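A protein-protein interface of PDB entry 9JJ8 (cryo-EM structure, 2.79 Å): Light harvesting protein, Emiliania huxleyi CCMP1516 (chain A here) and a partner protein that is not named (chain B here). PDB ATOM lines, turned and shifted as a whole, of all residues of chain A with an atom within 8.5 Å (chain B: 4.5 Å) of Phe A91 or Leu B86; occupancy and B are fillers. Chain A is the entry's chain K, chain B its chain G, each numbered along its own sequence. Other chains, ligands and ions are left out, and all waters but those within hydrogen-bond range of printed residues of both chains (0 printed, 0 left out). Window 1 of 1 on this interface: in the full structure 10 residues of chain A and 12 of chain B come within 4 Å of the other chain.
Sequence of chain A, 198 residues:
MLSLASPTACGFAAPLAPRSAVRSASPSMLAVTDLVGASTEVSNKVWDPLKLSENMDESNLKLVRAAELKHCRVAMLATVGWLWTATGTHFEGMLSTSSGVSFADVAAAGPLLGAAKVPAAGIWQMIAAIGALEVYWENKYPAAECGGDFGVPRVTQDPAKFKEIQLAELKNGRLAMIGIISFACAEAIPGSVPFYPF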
ATOM      1  N   TRP A  84     -17.989  11.507 -19.022  1.00  0.00           N
ATOM      2  CA  TRP A  84     -17.105  12.315 -18.184  1.00  0.00           C
ATOM      3  C   TRP A  84     -15.648  12.171 -18.606  1.00  0.00           C
ATOM      4  O   TRP A  84     -14.902  13.157 -18.635  1.00  0.00           O
ATOM      5  CB  TRP A  84     -17.272  11.931 -16.716  1.00  0.00           C
ATOM      6  CG  TRP A  84     -18.411  12.622 -16.038  1.00  0.00           C
ATOM      7  CD1 TRP A  84     -19.661  12.828 -16.540  1.00  0.00           C
ATOM      8  CD2 TRP A  84     -18.403  13.200 -14.729  1.00  0.00           C
ATOM      9  NE1 TRP A  84     -20.434  13.498 -15.623  1.00  0.00           N
ATOM     10  CE2 TRP A  84     -19.684  13.738 -14.503  1.00  0.00           C
ATOM     11  CE3 TRP A  84     -17.437  13.315 -13.725  1.00  0.00           C
ATOM     12  CZ2 TRP A  84     -20.024  14.381 -13.313  1.00  0.00           C
ATOM     13  CZ3 TRP A  84     -17.776  13.954 -12.547  1.00  0.00           C
ATOM     14  CH2 TRP A  84     -19.058  14.478 -12.352  1.00  0.00           C
ATOM     15  N   GLY A  88     -13.308  14.925 -20.806  1.00  0.00           N
ATOM     16  CA  GLY A  88     -11.979  15.222 -20.325  1.00  0.00           C
ATOM     17  C   GLY A  88     -11.843  15.381 -18.828  1.00  0.00           C
ATOM     18  O   GLY A  88     -10.717  15.396 -18.332  1.00  0.00           O
ATOM     19  N   THR A  89     -12.974  15.454 -18.111  1.00  0.00           N
ATOM     20  CA  THR A  89     -13.100  16.050 -16.777  1.00  0.00           C
ATOM     21  C   THR A  89     -12.024  15.674 -15.761  1.00  0.00           C
ATOM     22  O   THR A  89     -11.231  16.536 -15.371  1.00  0.00           O
ATOM     23  CB  THR A  89     -14.466  15.684 -16.190  1.00  0.00           C
ATOM     24  OG1 THR A  89     -15.490  15.932 -17.161  1.00  0.00           O
ATOM     25  CG2 THR A  89     -14.750  16.502 -14.943  1.00  0.00           C
ATOM     26  N   HIS A  90     -11.994  14.402 -15.343  1.00  0.00           N
ATOM     27  CA  HIS A  90     -10.993  13.765 -14.476  1.00  0.00           C
ATOM     28  C   HIS A  90     -10.794  14.423 -13.105  1.00  0.00           C
ATOM     29  O   HIS A  90     -11.279  15.527 -12.841  1.00  0.00           O
ATOM     30  CB  HIS A  90      -9.651  13.587 -15.224  1.00  0.00           C
ATOM     31  CG  HIS A  90      -8.785  14.810 -15.312  1.00  0.00           C
ATOM     32  ND1 HIS A  90      -8.033  15.280 -14.256  1.00  0.00           N
ATOM     33  CD2 HIS A  90      -8.489  15.611 -16.363  1.00  0.00           C
ATOM     34  CE1 HIS A  90      -7.353  16.346 -14.640  1.00  0.00           C
ATOM     35  NE2 HIS A  90      -7.614  16.568 -15.915  1.00  0.00           N
ATOM     36  N   PHE A  91     -10.122  13.715 -12.198  1.00  0.00           N
ATOM     37  CA  PHE A  91      -9.809  14.251 -10.879  1.00  0.00           C
ATOM     38  C   PHE A  91      -8.467  14.977 -10.928  1.00  0.00           C
ATOM     39  O   PHE A  91      -7.790  15.010 -11.958  1.00  0.00           O
ATOM     40  CB  PHE A  91      -9.802  13.139  -9.833  1.00  0.00           C
ATOM     41  CG  PHE A  91     -11.161  12.794  -9.294  1.00  0.00           C
ATOM     42  CD1 PHE A  91     -12.109  13.782  -9.082  1.00  0.00           C
ATOM     43  CD2 PHE A  91     -11.483  11.485  -8.980  1.00  0.00           C
ATOM     44  CE1 PHE A  91     -13.359  13.467  -8.579  1.00  0.00           C
ATOM     45  CE2 PHE A  91     -12.729  11.162  -8.476  1.00  0.00           C
ATOM     46  CZ  PHE A  91     -13.668  12.155  -8.276  1.00  0.00           C
ATOM     47  N   GLU A  92      -8.049  15.552  -9.805  1.00  0.00           N
ATOM     48  CA  GLU A  92      -6.772  16.252  -9.717  1.00  0.00           C
ATOM     49  C   GLU A  92      -5.943  15.615  -8.615  1.00  0.00           C
ATOM     50  O   GLU A  92      -6.390  15.531  -7.467  1.00  0.00           O
ATOM     51  CB  GLU A  92      -6.977  17.746  -9.451  1.00  0.00           C
ATOM     52  CG  GLU A  92      -7.587  18.499 -10.623  1.00  0.00           C
ATOM     53  CD  GLU A  92      -7.880  19.950 -10.300  1.00  0.00           C
ATOM     54  OE1 GLU A  92      -7.757  20.334  -9.119  1.00  0.00           O
ATOM     55  OE2 GLU A  92      -8.233  20.707 -11.229  1.00  0.00           O
ATOM     56  N   GLY A  93      -4.750  15.171  -8.961  1.00  0.00           N
ATOM     57  CA  GLY A  93      -3.874  14.512  -8.015  1.00  0.00           C
ATOM     58  C   GLY A  93      -3.085  13.416  -8.710  1.00  0.00           C
ATOM     59  O   GLY A  93      -2.850  13.476  -9.914  1.00  0.00           O
ATOM     60  N   MET A  94      -2.689  12.416  -7.924  1.00  0.00           N
ATOM     61  CA  MET A  94      -1.885  11.308  -8.421  1.00  0.00           C
ATOM     62  C   MET A  94      -2.598  10.017  -8.049  1.00  0.00           C
ATOM     63  O   MET A  94      -2.885   9.786  -6.870  1.00  0.00           O
ATOM     64  CB  MET A  94      -0.476  11.349  -7.826  1.00  0.00           C
ATOM     65  CG  MET A  94       0.599  10.773  -8.722  1.00  0.00           C
ATOM     66  SD  MET A  94       1.120  12.079  -9.858  1.00  0.00           S
ATOM     67  CE  MET A  94       2.314  11.231 -10.881  1.00  0.00           C
ATOM     68  N   LEU A  95      -2.892   9.183  -9.051  1.00  0.00           N
ATOM     69  CA  LEU A  95      -3.689   7.983  -8.806  1.00  0.00           C
ATOM     70  C   LEU A  95      -2.899   6.931  -8.035  1.00  0.00           C
ATOM     71  O   LEU A  95      -3.465   6.202  -7.213  1.00  0.00           O
ATOM     72  CB  LEU A  95      -4.203   7.415 -10.131  1.00  0.00           C
ATOM     73  CG  LEU A  95      -5.105   6.179 -10.111  1.00  0.00           C
ATOM     74  CD1 LEU A  95      -6.275   6.362  -9.157  1.00  0.00           C
ATOM     75  CD2 LEU A  95      -5.601   5.856 -11.512  1.00  0.00           C
ATOM     76  N   SER A 102      -1.060   9.832 -13.157  1.00  0.00           N
ATOM     77  CA  SER A 102      -2.016  10.795 -12.640  1.00  0.00           C
ATOM     78  C   SER A 102      -3.380  10.564 -13.281  1.00  0.00           C
ATOM     79  O   SER A 102      -3.520   9.800 -14.238  1.00  0.00           O
ATOM     80  CB  SER A 102      -1.543  12.226 -12.898  1.00  0.00           C
ATOM     81  OG  SER A 102      -1.540  12.521 -14.283  1.00  0.00           O
ATOM     82  N   PHE A 103      -4.399  11.226 -12.724  1.00  0.00           N
ATOM     83  CA  PHE A 103      -5.725  11.178 -13.332  1.00  0.00           C
ATOM     84  C   PHE A 103      -5.729  11.833 -14.706  1.00  0.00           C
ATOM     85  O   PHE A 103      -6.479  11.412 -15.596  1.00  0.00           O
ATOM     86  CB  PHE A 103      -6.751  11.851 -12.419  1.00  0.00           C
ATOM     87  CG  PHE A 103      -7.006  11.113 -11.134  1.00  0.00           C
ATOM     88  CD1 PHE A 103      -7.941  10.092 -11.080  1.00  0.00           C
ATOM     89  CD2 PHE A 103      -6.317  11.446  -9.979  1.00  0.00           C
ATOM     90  CE1 PHE A 103      -8.182   9.413  -9.898  1.00  0.00           C
ATOM     91  CE2 PHE A 103      -6.552  10.770  -8.794  1.00  0.00           C
ATOM     92  CZ  PHE A 103      -7.486   9.755  -8.755  1.00  0.00           C
ATOM     93  N   ALA A 104      -4.892  12.857 -14.898  1.00  0.00           N
ATOM     94  CA  ALA A 104      -4.744  13.467 -16.216  1.00  0.00           C
ATOM     95  C   ALA A 104      -4.105  12.498 -17.203  1.00  0.00           C
ATOM     96  O   ALA A 104      -4.446  12.500 -18.391  1.00  0.00           O
ATOM     97  CB  ALA A 104      -3.919  14.748 -16.109  1.00  0.00           C
ATOM     98  N   ASP A 105      -3.167  11.671 -16.730  1.00  0.00           N
ATOM     99  CA  ASP A 105      -2.562  10.656 -17.590  1.00  0.00           C
ATOM    100  C   ASP A 105      -3.585   9.613 -18.017  1.00  0.00           C
ATOM    101  O   ASP A 105      -3.568   9.145 -19.162  1.00  0.00           O
ATOM    102  CB  ASP A 105      -1.390   9.990 -16.871  1.00  0.00           C
ATOM    103  CG  ASP A 105      -0.213  10.925 -16.679  1.00  0.00           C
ATOM    104  OD1 ASP A 105      -0.033  11.838 -17.511  1.00  0.00           O
ATOM    105  OD2 ASP A 105       0.533  10.746 -15.693  1.00  0.00           O
ATOM    106  N   VAL A 106      -4.475   9.224 -17.101  1.00  0.00           N
ATOM    107  CA  VAL A 106      -5.528   8.267 -17.427  1.00  0.00           C
ATOM    108  C   VAL A 106      -6.523   8.874 -18.409  1.00  0.00           C
ATOM    109  O   VAL A 106      -6.948   8.221 -19.370  1.00  0.00           O
ATOM    110  CB  VAL A 106      -6.218   7.786 -16.136  1.00  0.00           C
ATOM    111  CG1 VAL A 106      -7.355   6.835 -16.449  1.00  0.00           C
ATOM    112  CG2 VAL A 106      -5.209   7.117 -15.219  1.00  0.00           C
ATOM    113  N   ALA A 107      -6.902  10.136 -18.189  1.00  0.00           N
ATOM    114  CA  ALA A 107      -7.900  10.772 -19.046  1.00  0.00           C
ATOM    115  C   ALA A 107      -7.346  11.074 -20.434  1.00  0.00           C
ATOM    116  O   ALA A 107      -8.079  11.006 -21.427  1.00  0.00           O
ATOM    117  CB  ALA A 107      -8.416  12.050 -18.389  1.00  0.00           C
ATOM    118  N   VAL B  82     -15.403  19.562  -3.000  1.00  0.00           N
ATOM    119  CA  VAL B  82     -15.291  18.874  -4.283  1.00  0.00           C
ATOM    120  C   VAL B  82     -14.597  19.746  -5.329  1.00  0.00           C
ATOM    121  O   VAL B  82     -13.845  19.236  -6.170  1.00  0.00           O
ATOM    122  CB  VAL B  82     -16.691  18.397  -4.722  1.00  0.00           C
ATOM    123  CG1 VAL B  82     -16.758  18.076  -6.209  1.00  0.00           C
ATOM    124  CG2 VAL B  82     -17.070  17.168  -3.912  1.00  0.00           C
ATOM    125  N   GLN B  83     -14.781  21.073  -5.270  1.00  0.00           N
ATOM    126  CA  GLN B  83     -14.105  21.955  -6.222  1.00  0.00           C
ATOM    127  C   GLN B  83     -12.585  21.933  -6.089  1.00  0.00           C
ATOM    128  O   GLN B  83     -11.896  22.360  -7.023  1.00  0.00           O
ATOM    129  CB  GLN B  83     -14.574  23.404  -6.065  1.00  0.00           C
ATOM    130  CG  GLN B  83     -15.983  23.695  -6.535  1.00  0.00           C
ATOM    131  CD  GLN B  83     -16.519  24.975  -5.928  1.00  0.00           C
ATOM    132  OE1 GLN B  83     -15.804  25.970  -5.834  1.00  0.00           O
ATOM    133  NE2 GLN B  83     -17.757  24.942  -5.463  1.00  0.00           N
ATOM    134  N   SER B  84     -12.052  21.459  -4.961  1.00  0.00           N
ATOM    135  CA  SER B  84     -10.607  21.417  -4.771  1.00  0.00           C
ATOM    136  C   SER B  84      -9.944  20.364  -5.653  1.00  0.00           C
ATOM    137  O   SER B  84      -8.869  20.613  -6.210  1.00  0.00           O
ATOM    138  CB  SER B  84     -10.282  21.159  -3.300  1.00  0.00           C
ATOM    139  OG  SER B  84     -10.951  20.004  -2.827  1.00  0.00           O
ATOM    140  N   PHE B  85     -10.559  19.189  -5.797  1.00  0.00           N
ATOM    141  CA  PHE B  85      -9.969  18.117  -6.589  1.00  0.00           C
ATOM    142  C   PHE B  85     -10.768  17.760  -7.836  1.00  0.00           C
ATOM    143  O   PHE B  85     -10.336  16.885  -8.594  1.00  0.00           O
ATOM    144  CB  PHE B  85      -9.759  16.857  -5.729  1.00  0.00           C
ATOM    145  CG  PHE B  85     -11.011  16.336  -5.063  1.00  0.00           C
ATOM    146  CD1 PHE B  85     -11.859  15.458  -5.724  1.00  0.00           C
ATOM    147  CD2 PHE B  85     -11.319  16.699  -3.762  1.00  0.00           C
ATOM    148  CE1 PHE B  85     -12.999  14.973  -5.110  1.00  0.00           C
ATOM    149  CE2 PHE B  85     -12.456  16.213  -3.142  1.00  0.00           C
ATOM    150  CZ  PHE B  85     -13.297  15.352  -3.817  1.00  0.00           C
ATOM    151  N   LEU B  86     -11.911  18.399  -8.072  1.00  0.00           N
ATOM    152  CA  LEU B  86     -12.706  18.134  -9.263  1.00  0.00           C
ATOM    153  C   LEU B  86     -13.089  19.453  -9.913  1.00  0.00           C
ATOM    154  O   LEU B  86     -13.511  20.391  -9.231  1.00  0.00           O
ATOM    155  CB  LEU B  86     -13.967  17.323  -8.934  1.00  0.00           C
ATOM    156  CG  LEU B  86     -14.870  16.968 -10.119  1.00  0.00           C
ATOM    157  CD1 LEU B  86     -14.099  16.171 -11.157  1.00  0.00           C
ATOM    158  CD2 LEU B  86     -16.097  16.201  -9.655  1.00  0.00           C
ATOM    159  N   ARG B  87     -12.941  19.519 -11.234  1.00  0.00           N
ATOM    160  CA  ARG B  87     -13.236  20.733 -11.977  1.00  0.00           C
ATOM    161  C   ARG B  87     -13.842  20.347 -13.318  1.00  0.00           C
ATOM    162  O   ARG B  87     -13.425  19.360 -13.928  1.00  0.00           O
ATOM    163  CB  ARG B  87     -11.969  21.573 -12.172  1.00  0.00           C
ATOM    164  CG  ARG B  87     -12.221  23.062 -12.252  1.00  0.00           C
ATOM    165  CD  ARG B  87     -12.719  23.606 -10.921  1.00  0.00           C
ATOM    166  NE  ARG B  87     -11.756  23.434  -9.841  1.00  0.00           N
ATOM    167  CZ  ARG B  87     -10.857  24.343  -9.491  1.00  0.00           C
ATOM    168  NH1 ARG B  87     -10.764  25.501 -10.121  1.00  0.00           N
ATOM    169  NH2 ARG B  87     -10.033  24.084  -8.480  1.00  0.00           N
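Printed residues of chain A that touch a printed residue of chain B: Thr A89, His A90, Phe A91 and Glu A92.
Hydrophobic or aromatic side chains of chain A within 4 Å of the printed part of chain B: Phe A91.
Of the 6 printed residues of chain B, 4 touch a printed residue of chain A.
Printed residues of chain B that touch a printed residue of chain A: Ser B84, Phe B85, Leu B86 and Arg B87.
Among the printed residues, no Asp or Glu carboxylate lies within 4 Å of a Lys or Arg side-chain nitrogen of the other chain.
Of the printed residues of chain A, Arg B87 touches Thr A89 (3.3 Å) and Glu A92 (3.9 Å).
Of the printed residues of chain B, Thr A89 touches Leu B86 (3.9 Å) and Arg B87 (3.3 Å).
Gln B83 touches none of the printed residues of chain A.
The nearest residue of chain A that does not touch Leu B86 is Trp A84 (4.03 Å).
The nearest printed residue of chain A that does not touch Arg B87 is His A90 (4.5 Å).
O of Gln B83 lies within hydrogen-bond range of NH2 of Arg B87, 2.9 Å away.
O of Trp A84 lies within hydrogen-bond range of N of Thr A89 (3.0 Å).
CG2 of Thr A89 touches CD1 of Leu B86, 3.9 Å away.
O of Arg B87 touches CG2 of Thr A89, 3.3 Å away.
Leu B86 touches His A90 (CD1 to O, 3.3 Å).
CA of Phe A91 touches O of Phe B85 (3.5 Å).
Phe A91 touches Leu B86.
CB of Arg B87 touches OE2 of Glu A92 (3.9 Å).
The backbone NH (N) of Glu A92 sits at hydrogen-bond distance from the backbone carbonyl oxygen (O) of Phe B85, 2.9 Å away.
The side-chain carboxylate (OE1) of Glu A92 lies close to the backbone carbonyl oxygen (O) of Ser B84 (3.1 Å).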
